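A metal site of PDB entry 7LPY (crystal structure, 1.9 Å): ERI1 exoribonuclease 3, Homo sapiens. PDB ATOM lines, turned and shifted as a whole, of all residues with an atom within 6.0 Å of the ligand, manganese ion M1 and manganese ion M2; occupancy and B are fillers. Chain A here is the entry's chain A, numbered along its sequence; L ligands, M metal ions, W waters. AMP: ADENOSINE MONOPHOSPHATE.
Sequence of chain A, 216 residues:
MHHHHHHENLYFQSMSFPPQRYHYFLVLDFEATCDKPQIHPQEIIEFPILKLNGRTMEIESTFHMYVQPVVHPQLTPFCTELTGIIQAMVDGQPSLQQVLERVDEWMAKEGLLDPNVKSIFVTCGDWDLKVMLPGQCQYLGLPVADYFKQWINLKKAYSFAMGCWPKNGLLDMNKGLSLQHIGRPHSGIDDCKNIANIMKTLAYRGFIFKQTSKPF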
ATOM      1  N   ASP A  29     -26.730 -17.735 -29.599  1.00  0.00           N
ATOM      2  CA  ASP A  29     -26.691 -16.340 -29.177  1.00  0.00           C
ATOM      3  C   ASP A  29     -25.823 -16.275 -27.932  1.00  0.00           C
ATOM      4  O   ASP A  29     -26.272 -16.721 -26.870  1.00  0.00           O
ATOM      5  CB  ASP A  29     -28.090 -15.808 -28.870  1.00  0.00           C
ATOM      6  CG  ASP A  29     -28.099 -14.318 -28.598  1.00  0.00           C
ATOM      7  OD1 ASP A  29     -27.937 -13.561 -29.569  1.00  0.00           O
ATOM      8  OD2 ASP A  29     -28.266 -13.899 -27.428  1.00  0.00           O
ATOM      9  N   PHE A  30     -24.602 -15.764 -28.031  1.00  0.00           N
ATOM     10  CA  PHE A  30     -23.763 -15.645 -26.854  1.00  0.00           C
ATOM     11  C   PHE A  30     -24.270 -14.539 -25.942  1.00  0.00           C
ATOM     12  O   PHE A  30     -24.859 -13.553 -26.388  1.00  0.00           O
ATOM     13  CB  PHE A  30     -22.326 -15.297 -27.239  1.00  0.00           C
ATOM     14  CG  PHE A  30     -21.617 -16.340 -28.059  1.00  0.00           C
ATOM     15  CD1 PHE A  30     -21.642 -17.686 -27.687  1.00  0.00           C
ATOM     16  CD2 PHE A  30     -20.935 -15.968 -29.236  1.00  0.00           C
ATOM     17  CE1 PHE A  30     -20.980 -18.644 -28.444  1.00  0.00           C
ATOM     18  CE2 PHE A  30     -20.270 -16.918 -29.997  1.00  0.00           C
ATOM     19  CZ  PHE A  30     -20.282 -18.269 -29.587  1.00  0.00           C
ATOM     20  N   GLU A  31     -24.022 -14.685 -24.637  1.00  0.00           N
ATOM     21  CA  GLU A  31     -23.873 -13.511 -23.791  1.00  0.00           C
ATOM     22  C   GLU A  31     -22.410 -13.416 -23.368  1.00  0.00           C
ATOM     23  O   GLU A  31     -21.708 -14.434 -23.301  1.00  0.00           O
ATOM     24  CB  GLU A  31     -24.769 -13.537 -22.550  1.00  0.00           C
ATOM     25  CG  GLU A  31     -26.254 -13.677 -22.833  1.00  0.00           C
ATOM     26  CD  GLU A  31     -26.822 -12.564 -23.675  1.00  0.00           C
ATOM     27  OE1 GLU A  31     -26.361 -11.401 -23.554  1.00  0.00           O
ATOM     28  OE2 GLU A  31     -27.780 -12.857 -24.424  1.00  0.00           O
ATOM     29  N   ALA A  32     -21.953 -12.197 -23.106  1.00  0.00           N
ATOM     30  CA  ALA A  32     -20.553 -11.954 -22.809  1.00  0.00           C
ATOM     31  C   ALA A  32     -20.451 -10.964 -21.662  1.00  0.00           C
ATOM     32  O   ALA A  32     -21.387 -10.211 -21.395  1.00  0.00           O
ATOM     33  CB  ALA A  32     -19.802 -11.382 -24.039  1.00  0.00           C
ATOM     34  N   THR A  33     -19.290 -10.974 -20.990  1.00  0.00           N
ATOM     35  CA  THR A  33     -18.973  -9.911 -20.045  1.00  0.00           C
ATOM     36  C   THR A  33     -19.095  -8.553 -20.746  1.00  0.00           C
ATOM     37  O   THR A  33     -18.859  -8.430 -21.947  1.00  0.00           O
ATOM     38  CB  THR A  33     -17.549 -10.069 -19.502  1.00  0.00           C
ATOM     39  OG1 THR A  33     -16.632 -10.060 -20.593  1.00  0.00           O
ATOM     40  CG2 THR A  33     -17.391 -11.391 -18.739  1.00  0.00           C
ATOM     41  N   CYS A  34     -19.473  -7.545 -19.965  1.00  0.00           N
ATOM     42  CA  CYS A  34     -19.681  -6.205 -20.487  1.00  0.00           C
ATOM     43  C   CYS A  34     -19.636  -5.226 -19.326  1.00  0.00           C
ATOM     44  O   CYS A  34     -19.567  -5.621 -18.156  1.00  0.00           O
ATOM     45  CB  CYS A  34     -21.005  -6.107 -21.255  1.00  0.00           C
ATOM     46  SG  CYS A  34     -22.426  -6.734 -20.326  1.00  0.00           S
ATOM     47  N   ASP A  35     -19.689  -3.937 -19.670  1.00  0.00           N
ATOM     48  CA  ASP A  35     -19.665  -2.865 -18.692  1.00  0.00           C
ATOM     49  C   ASP A  35     -20.013  -1.573 -19.415  1.00  0.00           C
ATOM     50  O   ASP A  35     -20.152  -1.550 -20.652  1.00  0.00           O
ATOM     51  CB  ASP A  35     -18.297  -2.787 -17.988  1.00  0.00           C
ATOM     52  CG  ASP A  35     -18.366  -2.075 -16.645  1.00  0.00           C
ATOM     53  OD1 ASP A  35     -19.471  -1.644 -16.238  1.00  0.00           O
ATOM     54  OD2 ASP A  35     -17.319  -1.980 -15.972  1.00  0.00           O
ATOM     55  N   LYS A  36     -20.114  -0.493 -18.658  1.00  0.00           N
ATOM     56  CA  LYS A  36     -20.414   0.819 -19.216  1.00  0.00           C
ATOM     57  C   LYS A  36     -19.333   1.788 -18.780  1.00  0.00           C
ATOM     58  O   LYS A  36     -19.261   2.124 -17.593  1.00  0.00           O
ATOM     59  CB  LYS A  36     -21.783   1.301 -18.728  1.00  0.00           C
ATOM     60  CG  LYS A  36     -22.635   1.812 -19.842  1.00  0.00           C
ATOM     61  CD  LYS A  36     -23.184   0.587 -20.523  1.00  0.00           C
ATOM     62  CE  LYS A  36     -24.221   0.919 -21.547  1.00  0.00           C
ATOM     63  NZ  LYS A  36     -23.814   0.441 -22.910  1.00  0.00           N
ATOM     64  N   GLN A  38     -17.713  -0.045 -22.462  1.00  0.00           N
ATOM     65  CA  GLN A  38     -17.567  -1.478 -22.688  1.00  0.00           C
ATOM     66  C   GLN A  38     -16.293  -2.024 -22.070  1.00  0.00           C
ATOM     67  O   GLN A  38     -15.249  -1.354 -22.042  1.00  0.00           O
ATOM     68  CB  GLN A  38     -17.595  -1.766 -24.190  1.00  0.00           C
ATOM     69  CG  GLN A  38     -17.777  -3.234 -24.521  1.00  0.00           C
ATOM     70  CD  GLN A  38     -18.973  -3.841 -23.797  1.00  0.00           C
ATOM     71  OE1 GLN A  38     -18.876  -4.195 -22.626  1.00  0.00           O
ATOM     72  NE2 GLN A  38     -20.099  -3.934 -24.488  1.00  0.00           N
ATOM     73  N   GLN A  42     -13.992  -8.475 -24.102  1.00  0.00           N
ATOM     74  CA  GLN A  42     -15.183  -9.219 -23.727  1.00  0.00           C
ATOM     75  C   GLN A  42     -14.888 -10.711 -23.747  1.00  0.00           C
ATOM     76  O   GLN A  42     -13.985 -11.182 -24.457  1.00  0.00           O
ATOM     77  CB  GLN A  42     -16.348  -8.926 -24.655  1.00  0.00           C
ATOM     78  CG  GLN A  42     -16.844  -7.493 -24.613  1.00  0.00           C
ATOM     79  CD  GLN A  42     -18.120  -7.323 -25.396  1.00  0.00           C
ATOM     80  OE1 GLN A  42     -18.086  -6.986 -26.572  1.00  0.00           O
ATOM     81  NE2 GLN A  42     -19.243  -7.564 -24.740  1.00  0.00           N
ATOM     82  N   ILE A  45     -19.808 -15.682 -21.669  1.00  0.00           N
ATOM     83  CA  ILE A  45     -20.247 -16.264 -20.401  1.00  0.00           C
ATOM     84  C   ILE A  45     -21.486 -17.136 -20.533  1.00  0.00           C
ATOM     85  O   ILE A  45     -21.875 -17.775 -19.553  1.00  0.00           O
ATOM     86  CB  ILE A  45     -20.506 -15.173 -19.325  1.00  0.00           C
ATOM     87  CG1 ILE A  45     -21.562 -14.178 -19.807  1.00  0.00           C
ATOM     88  CG2 ILE A  45     -19.210 -14.455 -18.972  1.00  0.00           C
ATOM     89  CD1 ILE A  45     -21.920 -13.110 -18.781  1.00  0.00           C
ATOM     90  N   PHE A  78     -23.395  -3.983 -14.239  1.00  0.00           N
ATOM     91  CA  PHE A  78     -24.093  -3.782 -15.512  1.00  0.00           C
ATOM     92  C   PHE A  78     -24.313  -5.102 -16.232  1.00  0.00           C
ATOM     93  O   PHE A  78     -25.391  -5.355 -16.781  1.00  0.00           O
ATOM     94  CB  PHE A  78     -23.315  -2.820 -16.410  1.00  0.00           C
ATOM     95  CG  PHE A  78     -23.932  -2.657 -17.771  1.00  0.00           C
ATOM     96  CD1 PHE A  78     -24.946  -1.719 -17.975  1.00  0.00           C
ATOM     97  CD2 PHE A  78     -23.538  -3.455 -18.823  1.00  0.00           C
ATOM     98  CE1 PHE A  78     -25.536  -1.584 -19.225  1.00  0.00           C
ATOM     99  CE2 PHE A  78     -24.121  -3.335 -20.076  1.00  0.00           C
ATOM    100  CZ  PHE A  78     -25.123  -2.386 -20.274  1.00  0.00           C
ATOM    101  N   LEU A  82     -27.925  -6.486 -17.184  1.00  0.00           N
ATOM    102  CA  LEU A  82     -28.293  -6.674 -18.580  1.00  0.00           C
ATOM    103  C   LEU A  82     -28.720  -8.119 -18.848  1.00  0.00           C
ATOM    104  O   LEU A  82     -29.812  -8.369 -19.377  1.00  0.00           O
ATOM    105  CB  LEU A  82     -27.129  -6.292 -19.488  1.00  0.00           C
ATOM    106  CG  LEU A  82     -27.426  -6.416 -20.986  1.00  0.00           C
ATOM    107  CD1 LEU A  82     -28.383  -5.303 -21.438  1.00  0.00           C
ATOM    108  CD2 LEU A  82     -26.128  -6.367 -21.786  1.00  0.00           C
ATOM    109  N   THR A  83     -27.871  -9.083 -18.502  1.00  0.00           N
ATOM    110  CA  THR A  83     -28.086 -10.465 -18.909  1.00  0.00           C
ATOM    111  C   THR A  83     -28.856 -11.282 -17.896  1.00  0.00           C
ATOM    112  O   THR A  83     -29.380 -12.351 -18.261  1.00  0.00           O
ATOM    113  CB  THR A  83     -26.747 -11.151 -19.165  1.00  0.00           C
ATOM    114  OG1 THR A  83     -26.030 -11.239 -17.933  1.00  0.00           O
ATOM    115  CG2 THR A  83     -25.917 -10.360 -20.193  1.00  0.00           C
ATOM    116  N   CYS A 124     -28.546 -13.761 -34.537  1.00  0.00           N
ATOM    117  CA  CYS A 124     -29.167 -12.455 -34.743  1.00  0.00           C
ATOM    118  C   CYS A 124     -28.050 -11.453 -34.949  1.00  0.00           C
ATOM    119  O   CYS A 124     -27.470 -10.939 -33.982  1.00  0.00           O
ATOM    120  CB  CYS A 124     -30.045 -12.053 -33.552  1.00  0.00           C
ATOM    121  SG  CYS A 124     -31.007 -10.513 -33.857  1.00  0.00           S
ATOM    122  N   TRP A 127     -22.373 -10.538 -35.199  1.00  0.00           N
ATOM    123  CA  TRP A 127     -21.388 -10.343 -34.126  1.00  0.00           C
ATOM    124  C   TRP A 127     -20.889 -11.670 -33.534  1.00  0.00           C
ATOM    125  O   TRP A 127     -19.684 -11.832 -33.281  1.00  0.00           O
ATOM    126  CB  TRP A 127     -21.992  -9.475 -33.036  1.00  0.00           C
ATOM    127  CG  TRP A 127     -21.104  -9.237 -31.831  1.00  0.00           C
ATOM    128  CD1 TRP A 127     -20.049  -8.353 -31.752  1.00  0.00           C
ATOM    129  CD2 TRP A 127     -21.203  -9.858 -30.541  1.00  0.00           C
ATOM    130  NE1 TRP A 127     -19.485  -8.410 -30.503  1.00  0.00           N
ATOM    131  CE2 TRP A 127     -20.176  -9.321 -29.744  1.00  0.00           C
ATOM    132  CE3 TRP A 127     -22.063 -10.817 -29.997  1.00  0.00           C
ATOM    133  CZ2 TRP A 127     -19.987  -9.702 -28.423  1.00  0.00           C
ATOM    134  CZ3 TRP A 127     -21.863 -11.205 -28.684  1.00  0.00           C
ATOM    135  CH2 TRP A 127     -20.847 -10.643 -27.912  1.00  0.00           C
ATOM    136  N   ASP A 128     -21.790 -12.622 -33.274  1.00  0.00           N
ATOM    137  CA  ASP A 128     -21.399 -13.807 -32.505  1.00  0.00           C
ATOM    138  C   ASP A 128     -20.245 -14.572 -33.145  1.00  0.00           C
ATOM    139  O   ASP A 128     -19.239 -14.866 -32.493  1.00  0.00           O
ATOM    140  CB  ASP A 128     -22.610 -14.728 -32.330  1.00  0.00           C
ATOM    141  CG  ASP A 128     -23.746 -14.033 -31.637  1.00  0.00           C
ATOM    142  OD1 ASP A 128     -23.992 -14.347 -30.465  1.00  0.00           O
ATOM    143  OD2 ASP A 128     -24.374 -13.152 -32.269  1.00  0.00           O
ATOM    144  N   HIS A 186     -32.294 -10.538 -23.491  1.00  0.00           N
ATOM    145  CA  HIS A 186     -30.864 -10.550 -23.171  1.00  0.00           C
ATOM    146  C   HIS A 186     -30.447 -11.751 -22.333  1.00  0.00           C
ATOM    147  O   HIS A 186     -29.367 -11.743 -21.713  1.00  0.00           O
ATOM    148  CB  HIS A 186     -30.443  -9.240 -22.490  1.00  0.00           C
ATOM    149  CG  HIS A 186     -30.881  -8.021 -23.245  1.00  0.00           C
ATOM    150  ND1 HIS A 186     -30.213  -7.566 -24.367  1.00  0.00           N
ATOM    151  CD2 HIS A 186     -31.931  -7.195 -23.075  1.00  0.00           C
ATOM    152  CE1 HIS A 186     -30.835  -6.507 -24.847  1.00  0.00           C
ATOM    153  NE2 HIS A 186     -31.874  -6.258 -24.075  1.00  0.00           N
ATOM    154  N   SER A 187     -31.265 -12.787 -22.286  1.00  0.00           N
ATOM    155  CA  SER A 187     -30.812 -14.108 -21.897  1.00  0.00           C
ATOM    156  C   SER A 187     -30.401 -14.853 -23.164  1.00  0.00           C
ATOM    157  O   SER A 187     -31.141 -14.830 -24.162  1.00  0.00           O
ATOM    158  CB  SER A 187     -31.918 -14.869 -21.148  1.00  0.00           C
ATOM    159  OG  SER A 187     -31.642 -16.255 -21.115  1.00  0.00           O
ATOM    160  N   GLY A 188     -29.235 -15.491 -23.147  1.00  0.00           N
ATOM    161  CA  GLY A 188     -28.790 -16.167 -24.358  1.00  0.00           C
ATOM    162  C   GLY A 188     -29.773 -17.234 -24.812  1.00  0.00           C
ATOM    163  O   GLY A 188     -30.204 -17.260 -25.970  1.00  0.00           O
ATOM    164  N   ASP A 191     -32.985 -15.596 -26.027  1.00  0.00           N
ATOM    165  CA  ASP A 191     -32.774 -15.006 -27.337  1.00  0.00           C
ATOM    166  C   ASP A 191     -32.814 -16.093 -28.412  1.00  0.00           C
ATOM    167  O   ASP A 191     -33.453 -15.913 -29.460  1.00  0.00           O
ATOM    168  CB  ASP A 191     -31.451 -14.226 -27.366  1.00  0.00           C
ATOM    169  CG  ASP A 191     -31.555 -12.874 -26.651  1.00  0.00           C
ATOM    170  OD1 ASP A 191     -32.678 -12.446 -26.323  1.00  0.00           O
ATOM    171  OD2 ASP A 191     -30.499 -12.227 -26.424  1.00  0.00           O
HETATM  172  P   AMP L   1     -27.111  -9.552 -27.656  1.00  0.00           P
HETATM  173  O1P AMP L   1     -26.472  -9.365 -29.019  1.00  0.00           O
HETATM  174  O2P AMP L   1     -27.570 -10.957 -27.406  1.00  0.00           O
HETATM  175  O3P AMP L   1     -28.156  -8.518 -27.281  1.00  0.00           O
HETATM  176  O5' AMP L   1     -25.953  -9.232 -26.609  1.00  0.00           O
HETATM  177  C5' AMP L   1     -24.702  -9.911 -26.643  1.00  0.00           C
HETATM  178  C4' AMP L   1     -23.690  -9.270 -25.710  1.00  0.00           C
HETATM  179  O4' AMP L   1     -23.361  -7.939 -26.181  1.00  0.00           O
HETATM  180  C3' AMP L   1     -24.143  -9.062 -24.263  1.00  0.00           C
HETATM  181  O3' AMP L   1     -24.035 -10.245 -23.468  1.00  0.00           O
HETATM  182  C2' AMP L   1     -23.230  -7.927 -23.807  1.00  0.00           C
HETATM  183  O2' AMP L   1     -21.918  -8.419 -23.518  1.00  0.00           O
HETATM  184  C1' AMP L   1     -23.161  -7.075 -25.082  1.00  0.00           C
HETATM  185  N9  AMP L   1     -24.238  -6.067 -25.087  1.00  0.00           N
HETATM  186  C8  AMP L   1     -25.491  -6.256 -25.569  1.00  0.00           C
HETATM  187  N7  AMP L   1     -26.250  -5.135 -25.376  1.00  0.00           N
HETATM  188  C5  AMP L   1     -25.461  -4.228 -24.760  1.00  0.00           C
HETATM  189  C6  AMP L   1     -25.625  -2.844 -24.252  1.00  0.00           C
HETATM  190  N6  AMP L   1     -26.810  -2.194 -24.382  1.00  0.00           N
HETATM  191  N1  AMP L   1     -24.574  -2.265 -23.663  1.00  0.00           N
HETATM  192  C2  AMP L   1     -23.400  -2.899 -23.509  1.00  0.00           C
HETATM  193  N3  AMP L   1     -23.180  -4.141 -23.945  1.00  0.00           N
HETATM  194  C4  AMP L   1     -24.149  -4.851 -24.558  1.00  0.00           C
HETATM  195 MN    MN M   1     -28.556 -12.171 -26.306  1.00  0.00          MN
HETATM  196 MN    MN M   2     -27.064 -11.544 -29.567  1.00  0.00          MN
HETATM  197  O   HOH W   1     -29.241 -10.825 -30.091  1.00  0.00           O
HETATM  198  O   HOH W   2     -20.862  -6.209 -27.388  1.00  0.00           O
HETATM  199  O   HOH W   3     -25.133 -12.389 -28.953  1.00  0.00           O
HETATM  200  O   HOH W   4     -28.531 -10.571 -25.228  1.00  0.00           O
HETATM  201  O   HOH W   5     -29.136  -6.406 -28.855  1.00  0.00           O
HETATM  202  O   HOH W   6     -26.124 -11.717 -31.627  1.00  0.00           O
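The side-chain carboxylate of Asp 191 sits at hydrogen-bond distance from the backbone NH of His 186, at 3.4 Å.
The backbone NH of Ile 45 is in hydrogen-bond range of the backbone carbonyl oxygen of Glu 31, at 2.8 Å.
The side-chain sulfur (SG) of Cys 34 sits at hydrogen-bond distance from the backbone carbonyl oxygen (O) of Ala 32.
The backbone NH of Gly 188 sits close to the side-chain carboxylate of Glu 31.
OE1 of Gln 38 sits at hydrogen-bond distance from N of Asp 35.
NE2 of Gln 42 is in hydrogen-bond range of O of Thr 33 (2.9 Å).
The backbone NH (N) of Phe 30 sits at hydrogen-bond distance from the side-chain carboxylate (OD1) of Asp 128.
Merely in contact with manganese ion M1: Phe 30 (3.9 Å).
Of the 21 residues printed, 4 come within 4 Å of manganese ion M1.
The backbone carbonyl oxygen (O) of Thr 33 lies within hydrogen-bond range of an oxygen (O2') of the ligand, at 3.4 Å.
NE2 of Gln 42 is in hydrogen-bond range of O2' of the ligand (3.1 Å).
N of Ala 32 lies within hydrogen-bond range of O3' of the ligand (2.9 Å).
The backbone carbonyl oxygen of Ala 32 is in hydrogen-bond range of an oxygen (O2') of the ligand (2.8 Å).
N1 of the ligand sits at hydrogen-bond distance from NZ of Lys 36.
A nitrogen (N3) of the ligand sits at hydrogen-bond distance from the side-chain amide nitrogen (NE2) of Gln 38 (3.1 Å).
The side-chain sulfur of Cys 34 sits close to an oxygen (O2') of the ligand.
Within 4 Å of manganese ion M2: Asp 29.
Manganese ion M2 is bound by water W3 (2.2 Å), the side-chain carboxylate (OD1) of Asp 29 (2.2 Å), water W6 (2.3 Å), an oxygen (O2P) of the ligand (2.3 Å), an oxygen (O1P) of the ligand (2.3 Å) and water W1 (2.4 Å).
O of Phe 30 touches C5' of the ligand, 3.7 Å away.
Phe 78 touches the ligand (CZ to N1, 3.4 Å).
CD2 of Leu 82 touches C5 of the ligand, at 3.7 Å.
Thr 83 touches the ligand (CG2 to O3', 3.8 Å).
Trp 127 touches the ligand.
ND1 of His 186 touches O3P of the ligand (3.7 Å).
Of the 21 residues printed, 15 come within 4 Å of the ligand.
The nearest printed residue that does not touch the ligand is Asp 35 (4.5 Å).
Water W4 bridges OE1 of Glu 31 (2.9 Å) and O3P of the ligand (2.9 Å).
Water W3 lies within hydrogen-bond range of the side-chain carboxylate (OD1) of Asp 128 (2.7 Å) and the backbone carbonyl oxygen (O) of Phe 30 (2.8 Å).
Water W2 lies within hydrogen-bond range of the side-chain amide oxygen of Gln 42 (3.0 Å) and an oxygen (O4') of the ligand (3.3 Å).
An oxygen (O2P) of the ligand is bound to manganese ion M1 (1.9 Å).
Manganese ion M1 is bound by water W4, at 1.9 Å.
OD2 of Asp 191 is bound to manganese ion M1.
Manganese ion M1 is bound by the side-chain carboxylate (OD2) of Asp 29, at 2.1 Å.
OE2 of Glu 31 is bound to manganese ion M1 (2.1 Å).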
